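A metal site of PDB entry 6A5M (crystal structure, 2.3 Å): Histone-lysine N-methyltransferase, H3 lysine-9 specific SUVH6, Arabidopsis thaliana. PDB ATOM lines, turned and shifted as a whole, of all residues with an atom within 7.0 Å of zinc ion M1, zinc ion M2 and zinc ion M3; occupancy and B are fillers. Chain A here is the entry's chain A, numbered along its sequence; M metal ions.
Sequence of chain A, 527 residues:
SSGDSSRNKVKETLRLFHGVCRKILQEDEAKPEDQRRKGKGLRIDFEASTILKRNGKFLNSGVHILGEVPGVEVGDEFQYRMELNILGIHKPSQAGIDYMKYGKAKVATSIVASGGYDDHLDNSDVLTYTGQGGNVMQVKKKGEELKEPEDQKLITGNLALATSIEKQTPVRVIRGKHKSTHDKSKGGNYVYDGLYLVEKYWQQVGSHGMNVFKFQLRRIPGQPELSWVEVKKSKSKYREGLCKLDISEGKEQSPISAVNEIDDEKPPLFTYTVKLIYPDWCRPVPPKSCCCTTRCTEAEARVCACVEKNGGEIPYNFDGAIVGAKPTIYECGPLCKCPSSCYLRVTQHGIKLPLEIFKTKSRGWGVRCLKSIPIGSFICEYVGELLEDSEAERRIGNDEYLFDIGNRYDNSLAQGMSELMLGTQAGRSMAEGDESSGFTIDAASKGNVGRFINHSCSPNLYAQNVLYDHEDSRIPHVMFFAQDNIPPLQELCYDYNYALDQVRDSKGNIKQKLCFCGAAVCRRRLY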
ATOM      1  N   LYS A 288      -6.473 -18.730  23.671  1.00  0.00           N
ATOM      2  CA  LYS A 288      -6.825 -18.610  22.265  1.00  0.00           C
ATOM      3  C   LYS A 288      -8.124 -19.341  22.020  1.00  0.00           C
ATOM      4  O   LYS A 288      -8.299 -20.477  22.438  1.00  0.00           O
ATOM      5  CB  LYS A 288      -5.704 -19.161  21.355  1.00  0.00           C
ATOM      6  CG  LYS A 288      -4.255 -18.794  21.789  1.00  0.00           C
ATOM      7  CD  LYS A 288      -4.053 -17.384  22.373  1.00  0.00           C
ATOM      8  CE  LYS A 288      -4.751 -16.267  21.600  1.00  0.00           C
ATOM      9  NZ  LYS A 288      -5.002 -15.108  22.497  1.00  0.00           N
ATOM     10  N   SER A 289      -9.028 -18.576  21.403  1.00  0.00           N
ATOM     11  CA  SER A 289     -10.448 -18.814  21.342  1.00  0.00           C
ATOM     12  C   SER A 289     -10.883 -19.660  20.164  1.00  0.00           C
ATOM     13  O   SER A 289     -10.067 -20.297  19.486  1.00  0.00           O
ATOM     14  CB  SER A 289     -11.213 -17.488  21.323  1.00  0.00           C
ATOM     15  OG  SER A 289     -11.364 -16.996  20.008  1.00  0.00           O
ATOM     16  N   CYS A 290     -12.184 -19.639  19.908  1.00  0.00           N
ATOM     17  CA  CYS A 290     -12.809 -20.557  18.977  1.00  0.00           C
ATOM     18  C   CYS A 290     -13.656 -19.862  17.932  1.00  0.00           C
ATOM     19  O   CYS A 290     -14.209 -18.789  18.171  1.00  0.00           O
ATOM     20  CB  CYS A 290     -13.652 -21.552  19.748  1.00  0.00           C
ATOM     21  SG  CYS A 290     -13.986 -23.050  18.821  1.00  0.00           S
ATOM     22  N   CYS A 291     -13.766 -20.490  16.767  1.00  0.00           N
ATOM     23  CA  CYS A 291     -14.545 -19.935  15.666  1.00  0.00           C
ATOM     24  C   CYS A 291     -15.548 -20.973  15.178  1.00  0.00           C
ATOM     25  O   CYS A 291     -15.402 -21.551  14.099  1.00  0.00           O
ATOM     26  CB  CYS A 291     -13.629 -19.509  14.527  1.00  0.00           C
ATOM     27  SG  CYS A 291     -13.025 -17.804  14.650  1.00  0.00           S
ATOM     28  N   CYS A 292     -16.577 -21.197  15.985  1.00  0.00           N
ATOM     29  CA  CYS A 292     -17.659 -22.121  15.675  1.00  0.00           C
ATOM     30  C   CYS A 292     -18.907 -21.541  16.324  1.00  0.00           C
ATOM     31  O   CYS A 292     -18.906 -21.214  17.499  1.00  0.00           O
ATOM     32  CB  CYS A 292     -17.355 -23.530  16.209  1.00  0.00           C
ATOM     33  SG  CYS A 292     -15.693 -24.195  15.838  1.00  0.00           S
ATOM     34  N   THR A 293     -19.970 -21.391  15.538  1.00  0.00           N
ATOM     35  CA  THR A 293     -21.190 -20.778  16.054  1.00  0.00           C
ATOM     36  C   THR A 293     -22.095 -21.796  16.730  1.00  0.00           C
ATOM     37  O   THR A 293     -23.095 -21.447  17.346  1.00  0.00           O
ATOM     38  CB  THR A 293     -21.971 -20.062  14.966  1.00  0.00           C
ATOM     39  OG1 THR A 293     -23.042 -19.315  15.557  1.00  0.00           O
ATOM     40  CG2 THR A 293     -22.539 -21.069  13.974  1.00  0.00           C
ATOM     41  N   THR A 294     -21.746 -23.073  16.588  1.00  0.00           N
ATOM     42  CA  THR A 294     -22.507 -24.118  17.230  1.00  0.00           C
ATOM     43  C   THR A 294     -21.587 -25.116  17.915  1.00  0.00           C
ATOM     44  O   THR A 294     -20.375 -24.905  17.960  1.00  0.00           O
ATOM     45  CB  THR A 294     -23.385 -24.853  16.239  1.00  0.00           C
ATOM     46  OG1 THR A 294     -24.180 -25.803  16.947  1.00  0.00           O
ATOM     47  CG2 THR A 294     -22.517 -25.577  15.206  1.00  0.00           C
ATOM     48  N   ARG A 295     -22.152 -26.204  18.434  1.00  0.00           N
ATOM     49  CA  ARG A 295     -21.354 -27.221  19.125  1.00  0.00           C
ATOM     50  C   ARG A 295     -20.158 -27.670  18.302  1.00  0.00           C
ATOM     51  O   ARG A 295     -20.300 -28.032  17.137  1.00  0.00           O
ATOM     52  CB  ARG A 295     -22.195 -28.455  19.486  1.00  0.00           C
ATOM     53  CG  ARG A 295     -23.509 -28.181  20.186  1.00  0.00           C
ATOM     54  CD  ARG A 295     -24.162 -29.493  20.555  1.00  0.00           C
ATOM     55  NE  ARG A 295     -25.343 -29.319  21.390  1.00  0.00           N
ATOM     56  CZ  ARG A 295     -25.930 -30.293  22.080  1.00  0.00           C
ATOM     57  NH1 ARG A 295     -27.002 -30.042  22.799  1.00  0.00           N
ATOM     58  NH2 ARG A 295     -25.432 -31.522  22.039  1.00  0.00           N
ATOM     59  N   CYS A 296     -18.983 -27.643  18.918  1.00  0.00           N
ATOM     60  CA  CYS A 296     -17.763 -28.071  18.239  1.00  0.00           C
ATOM     61  C   CYS A 296     -17.730 -29.570  18.086  1.00  0.00           C
ATOM     62  O   CYS A 296     -18.030 -30.315  19.020  1.00  0.00           O
ATOM     63  CB  CYS A 296     -16.520 -27.619  18.981  1.00  0.00           C
ATOM     64  SG  CYS A 296     -16.400 -25.859  19.072  1.00  0.00           S
ATOM     65  N   THR A 297     -17.393 -29.973  16.870  1.00  0.00           N
ATOM     66  CA  THR A 297     -17.233 -31.344  16.495  1.00  0.00           C
ATOM     67  C   THR A 297     -16.223 -31.486  15.359  1.00  0.00           C
ATOM     68  O   THR A 297     -16.045 -30.576  14.588  1.00  0.00           O
ATOM     69  CB  THR A 297     -18.582 -31.956  16.129  1.00  0.00           C
ATOM     70  OG1 THR A 297     -18.392 -33.117  15.325  1.00  0.00           O
ATOM     71  CG2 THR A 297     -19.408 -31.008  15.353  1.00  0.00           C
ATOM     72  N   VAL A 303     -12.332 -25.111  10.465  1.00  0.00           N
ATOM     73  CA  VAL A 303     -11.369 -25.305  11.543  1.00  0.00           C
ATOM     74  C   VAL A 303     -11.905 -24.966  12.929  1.00  0.00           C
ATOM     75  O   VAL A 303     -12.443 -23.906  13.136  1.00  0.00           O
ATOM     76  CB  VAL A 303     -10.097 -24.467  11.285  1.00  0.00           C
ATOM     77  CG1 VAL A 303      -9.128 -24.524  12.466  1.00  0.00           C
ATOM     78  CG2 VAL A 303      -9.395 -24.952  10.044  1.00  0.00           C
ATOM     79  N   CYS A 304     -11.688 -25.856  13.881  1.00  0.00           N
ATOM     80  CA  CYS A 304     -11.882 -25.521  15.283  1.00  0.00           C
ATOM     81  C   CYS A 304     -10.542 -25.637  16.014  1.00  0.00           C
ATOM     82  O   CYS A 304      -9.988 -26.730  16.142  1.00  0.00           O
ATOM     83  CB  CYS A 304     -12.920 -26.438  15.949  1.00  0.00           C
ATOM     84  SG  CYS A 304     -13.087 -26.158  17.733  1.00  0.00           S
ATOM     85  N   ALA A 305     -10.025 -24.496  16.467  1.00  0.00           N
ATOM     86  CA  ALA A 305      -8.726 -24.431  17.142  1.00  0.00           C
ATOM     87  C   ALA A 305      -8.686 -25.310  18.384  1.00  0.00           C
ATOM     88  O   ALA A 305      -7.666 -25.916  18.708  1.00  0.00           O
ATOM     89  CB  ALA A 305      -8.415 -23.003  17.526  1.00  0.00           C
ATOM     90  N   CYS A 306      -9.811 -25.381  19.084  1.00  0.00           N
ATOM     91  CA  CYS A 306      -9.861 -26.131  20.325  1.00  0.00           C
ATOM     92  C   CYS A 306      -9.769 -27.633  20.071  1.00  0.00           C
ATOM     93  O   CYS A 306      -9.209 -28.366  20.883  1.00  0.00           O
ATOM     94  CB  CYS A 306     -11.128 -25.749  21.097  1.00  0.00           C
ATOM     95  SG  CYS A 306     -11.153 -23.959  21.471  1.00  0.00           S
ATOM     96  N   VAL A 307     -10.267 -28.103  18.929  1.00  0.00           N
ATOM     97  CA  VAL A 307     -10.078 -29.499  18.533  1.00  0.00           C
ATOM     98  C   VAL A 307      -8.611 -29.803  18.203  1.00  0.00           C
ATOM     99  O   VAL A 307      -8.125 -30.913  18.468  1.00  0.00           O
ATOM    100  CB  VAL A 307     -10.961 -29.868  17.316  1.00  0.00           C
ATOM    101  CG1 VAL A 307     -10.658 -31.275  16.818  1.00  0.00           C
ATOM    102  CG2 VAL A 307     -12.432 -29.716  17.667  1.00  0.00           C
ATOM    103  N   LYS A 309      -6.109 -28.205  19.604  1.00  0.00           N
ATOM    104  CA  LYS A 309      -5.455 -28.207  20.913  1.00  0.00           C
ATOM    105  C   LYS A 309      -5.461 -29.614  21.513  1.00  0.00           C
ATOM    106  O   LYS A 309      -4.517 -30.016  22.180  1.00  0.00           O
ATOM    107  CB  LYS A 309      -6.146 -27.246  21.876  1.00  0.00           C
ATOM    108  CG  LYS A 309      -5.752 -25.792  21.724  1.00  0.00           C
ATOM    109  CD  LYS A 309      -6.575 -24.930  22.687  1.00  0.00           C
ATOM    110  CE  LYS A 309      -6.568 -23.462  22.253  1.00  0.00           C
ATOM    111  NZ  LYS A 309      -7.498 -22.649  23.081  1.00  0.00           N
ATOM    112  N   GLU A 331     -10.812 -27.539  26.977  1.00  0.00           N
ATOM    113  CA  GLU A 331     -12.215 -27.247  26.739  1.00  0.00           C
ATOM    114  C   GLU A 331     -12.353 -25.862  26.096  1.00  0.00           C
ATOM    115  O   GLU A 331     -11.420 -25.055  26.162  1.00  0.00           O
ATOM    116  CB  GLU A 331     -13.025 -27.311  28.047  1.00  0.00           C
ATOM    117  CG  GLU A 331     -13.383 -28.749  28.499  1.00  0.00           C
ATOM    118  CD  GLU A 331     -14.262 -28.775  29.751  1.00  0.00           C
ATOM    119  OE1 GLU A 331     -14.942 -27.767  30.027  1.00  0.00           O
ATOM    120  OE2 GLU A 331     -14.280 -29.794  30.466  1.00  0.00           O
ATOM    121  N   CYS A 332     -13.491 -25.590  25.481  1.00  0.00           N
ATOM    122  CA  CYS A 332     -13.739 -24.272  24.930  1.00  0.00           C
ATOM    123  C   CYS A 332     -13.872 -23.282  26.072  1.00  0.00           C
ATOM    124  O   CYS A 332     -14.357 -23.629  27.150  1.00  0.00           O
ATOM    125  CB  CYS A 332     -15.001 -24.256  24.048  1.00  0.00           C
ATOM    126  SG  CYS A 332     -14.730 -25.081  22.466  1.00  0.00           S
ATOM    127  N   GLY A 333     -13.414 -22.049  25.832  1.00  0.00           N
ATOM    128  CA  GLY A 333     -13.270 -21.070  26.891  1.00  0.00           C
ATOM    129  C   GLY A 333     -14.300 -19.959  26.808  1.00  0.00           C
ATOM    130  O   GLY A 333     -15.316 -20.102  26.130  1.00  0.00           O
ATOM    131  N   LEU A 335     -14.266 -16.993  25.475  1.00  0.00           N
ATOM    132  CA  LEU A 335     -14.371 -16.227  24.252  1.00  0.00           C
ATOM    133  C   LEU A 335     -14.556 -17.127  23.023  1.00  0.00           C
ATOM    134  O   LEU A 335     -14.470 -16.636  21.901  1.00  0.00           O
ATOM    135  CB  LEU A 335     -13.148 -15.327  24.065  1.00  0.00           C
ATOM    136  CG  LEU A 335     -12.953 -14.247  25.133  1.00  0.00           C
ATOM    137  CD1 LEU A 335     -11.885 -13.263  24.705  1.00  0.00           C
ATOM    138  CD2 LEU A 335     -14.248 -13.537  25.427  1.00  0.00           C
ATOM    139  N   CYS A 336     -14.792 -18.418  23.221  1.00  0.00           N
ATOM    140  CA  CYS A 336     -15.272 -19.265  22.119  1.00  0.00           C
ATOM    141  C   CYS A 336     -16.743 -18.934  21.825  1.00  0.00           C
ATOM    142  O   CYS A 336     -17.543 -18.800  22.759  1.00  0.00           O
ATOM    143  CB  CYS A 336     -15.099 -20.754  22.440  1.00  0.00           C
ATOM    144  SG  CYS A 336     -13.396 -21.313  22.646  1.00  0.00           S
ATOM    145  N   LYS A 337     -17.107 -18.801  20.561  1.00  0.00           N
ATOM    146  CA  LYS A 337     -18.476 -18.409  20.195  1.00  0.00           C
ATOM    147  C   LYS A 337     -19.471 -19.574  20.286  1.00  0.00           C
ATOM    148  O   LYS A 337     -20.648 -19.447  19.954  1.00  0.00           O
ATOM    149  CB  LYS A 337     -18.477 -17.799  18.802  1.00  0.00           C
ATOM    150  CG  LYS A 337     -17.389 -16.744  18.610  1.00  0.00           C
ATOM    151  CD  LYS A 337     -17.294 -16.286  17.169  1.00  0.00           C
ATOM    152  CE  LYS A 337     -16.299 -15.164  17.008  1.00  0.00           C
ATOM    153  NZ  LYS A 337     -15.932 -14.956  15.578  1.00  0.00           N
ATOM    154  N   CYS A 338     -18.969 -20.689  20.804  1.00  0.00           N
ATOM    155  CA  CYS A 338     -19.793 -21.869  21.027  1.00  0.00           C
ATOM    156  C   CYS A 338     -20.859 -21.638  22.056  1.00  0.00           C
ATOM    157  O   CYS A 338     -20.688 -20.878  23.003  1.00  0.00           O
ATOM    158  CB  CYS A 338     -18.933 -23.031  21.515  1.00  0.00           C
ATOM    159  SG  CYS A 338     -17.558 -23.364  20.432  1.00  0.00           S
ATOM    160  N   PRO A 339     -21.968 -22.335  21.866  1.00  0.00           N
ATOM    161  CA  PRO A 339     -23.038 -22.345  22.863  1.00  0.00           C
ATOM    162  C   PRO A 339     -22.598 -23.142  24.086  1.00  0.00           C
ATOM    163  O   PRO A 339     -21.622 -23.877  24.011  1.00  0.00           O
ATOM    164  CB  PRO A 339     -24.191 -23.026  22.134  1.00  0.00           C
ATOM    165  CG  PRO A 339     -23.510 -23.946  21.189  1.00  0.00           C
ATOM    166  CD  PRO A 339     -22.281 -23.210  20.728  1.00  0.00           C
ATOM    167  N   CYS A 342     -21.848 -26.971  23.752  1.00  0.00           N
ATOM    168  CA  CYS A 342     -20.725 -27.484  22.972  1.00  0.00           C
ATOM    169  C   CYS A 342     -20.144 -28.753  23.613  1.00  0.00           C
ATOM    170  O   CYS A 342     -20.106 -28.880  24.844  1.00  0.00           O
ATOM    171  CB  CYS A 342     -19.629 -26.428  22.832  1.00  0.00           C
ATOM    172  SG  CYS A 342     -18.108 -27.045  22.073  1.00  0.00           S
ATOM    173  N   TYR A 343     -19.700 -29.688  22.768  1.00  0.00           N
ATOM    174  CA  TYR A 343     -19.212 -30.986  23.256  1.00  0.00           C
ATOM    175  C   TYR A 343     -17.878 -30.848  23.994  1.00  0.00           C
ATOM    176  O   TYR A 343     -17.460 -31.755  24.728  1.00  0.00           O
ATOM    177  CB  TYR A 343     -19.062 -31.975  22.097  1.00  0.00           C
ATOM    178  CG  TYR A 343     -20.371 -32.324  21.390  1.00  0.00           C
ATOM    179  CD1 TYR A 343     -21.429 -32.890  22.098  1.00  0.00           C
ATOM    180  CD2 TYR A 343     -20.525 -32.104  20.030  1.00  0.00           C
ATOM    181  CE1 TYR A 343     -22.625 -33.214  21.464  1.00  0.00           C
ATOM    182  CE2 TYR A 343     -21.717 -32.429  19.382  1.00  0.00           C
ATOM    183  CZ  TYR A 343     -22.764 -32.985  20.107  1.00  0.00           C
ATOM    184  OH  TYR A 343     -23.942 -33.317  19.477  1.00  0.00           O
ATOM    185  N   LEU A 344     -17.218 -29.714  23.768  1.00  0.00           N
ATOM    186  CA  LEU A 344     -15.971 -29.382  24.430  1.00  0.00           C
ATOM    187  C   LEU A 344     -16.228 -28.522  25.656  1.00  0.00           C
ATOM    188  O   LEU A 344     -15.323 -27.872  26.139  1.00  0.00           O
ATOM    189  CB  LEU A 344     -15.034 -28.630  23.476  1.00  0.00           C
ATOM    190  CG  LEU A 344     -14.249 -29.475  22.473  1.00  0.00           C
ATOM    191  CD1 LEU A 344     -13.010 -28.736  22.021  1.00  0.00           C
ATOM    192  CD2 LEU A 344     -13.867 -30.784  23.123  1.00  0.00           C
ATOM    193  N   ARG A 345     -17.461 -28.498  26.126  1.00  0.00           N
ATOM    194  CA  ARG A 345     -17.773 -27.785  27.361  1.00  0.00           C
ATOM    195  C   ARG A 345     -18.398 -28.758  28.348  1.00  0.00           C
ATOM    196  O   ARG A 345     -19.588 -29.066  28.241  1.00  0.00           O
ATOM    197  CB  ARG A 345     -18.715 -26.602  27.114  1.00  0.00           C
ATOM    198  CG  ARG A 345     -18.140 -25.463  26.280  1.00  0.00           C
ATOM    199  CD  ARG A 345     -19.150 -24.339  26.223  1.00  0.00           C
ATOM    200  NE  ARG A 345     -18.843 -23.267  25.280  1.00  0.00           N
ATOM    201  CZ  ARG A 345     -18.107 -22.192  25.573  1.00  0.00           C
ATOM    202  NH1 ARG A 345     -17.563 -22.044  26.780  1.00  0.00           N
ATOM    203  NH2 ARG A 345     -17.909 -21.267  24.632  1.00  0.00           N
HETATM  204 ZN    ZN M   1     -16.809 -25.204  21.447  1.00  0.00          ZN
HETATM  205 ZN    ZN M   2     -13.396 -23.329  21.378  1.00  0.00          ZN
HETATM  206 ZN    ZN M   3     -14.852 -24.841  18.020  1.00  0.00          ZN
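The side-chain sulfur (SG) of Cys 304 lies close to the backbone NH (N) of Cys 306 (3.6 Å). The backbone NH (N) of Val 307 lies close to the side-chain sulfur (SG) of Cys 304 (3.6 Å). The backbone NH (N) of Cys 338 sits at hydrogen-bond distance from the backbone carbonyl oxygen (O) of Cys 292 (3.3 Å). O of Cys 338 lies within hydrogen-bond range of NH2 of Arg 345, at 3.2 Å. The backbone NH of Cys 332 is in hydrogen-bond range of the backbone carbonyl oxygen of Leu 344 (3.0 Å). The backbone NH (N) of Leu 344 sits close to the side-chain sulfur (SG) of Cys 342. The side-chain sulfur (SG) of Cys 336 sits close to the backbone NH (N) of Gly 333. O of Cys 336 sits at hydrogen-bond distance from NH2 of Arg 345 (3.1 Å).
Zinc ion M2 is bound by SG of Cys 306 (2.3 Å), SG of Cys 336 (2.4 Å), SG of Cys 332 (2.5 Å) and SG of Cys 290 (2.6 Å).
Zinc ion M3 is bound by SG of Cys 296, SG of Cys 290, SG of Cys 304 and SG of Cys 292.
Of the 28 residues printed, 4 come within 4 Å of zinc ion M2.
Along chain A the residues within 4 Å of zinc ion M3 span positions 290 to 338. The nearest printed residue that does not touch zinc ion M3 is Cys 332 (4.5 Å).
Zinc ion M1 is bound by the side-chain sulfur of Cys 338 (2.2 Å), the side-chain sulfur of Cys 332 (2.3 Å), the side-chain sulfur of Cys 342 (2.3 Å) and the side-chain sulfur of Cys 296 (2.5 Å).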
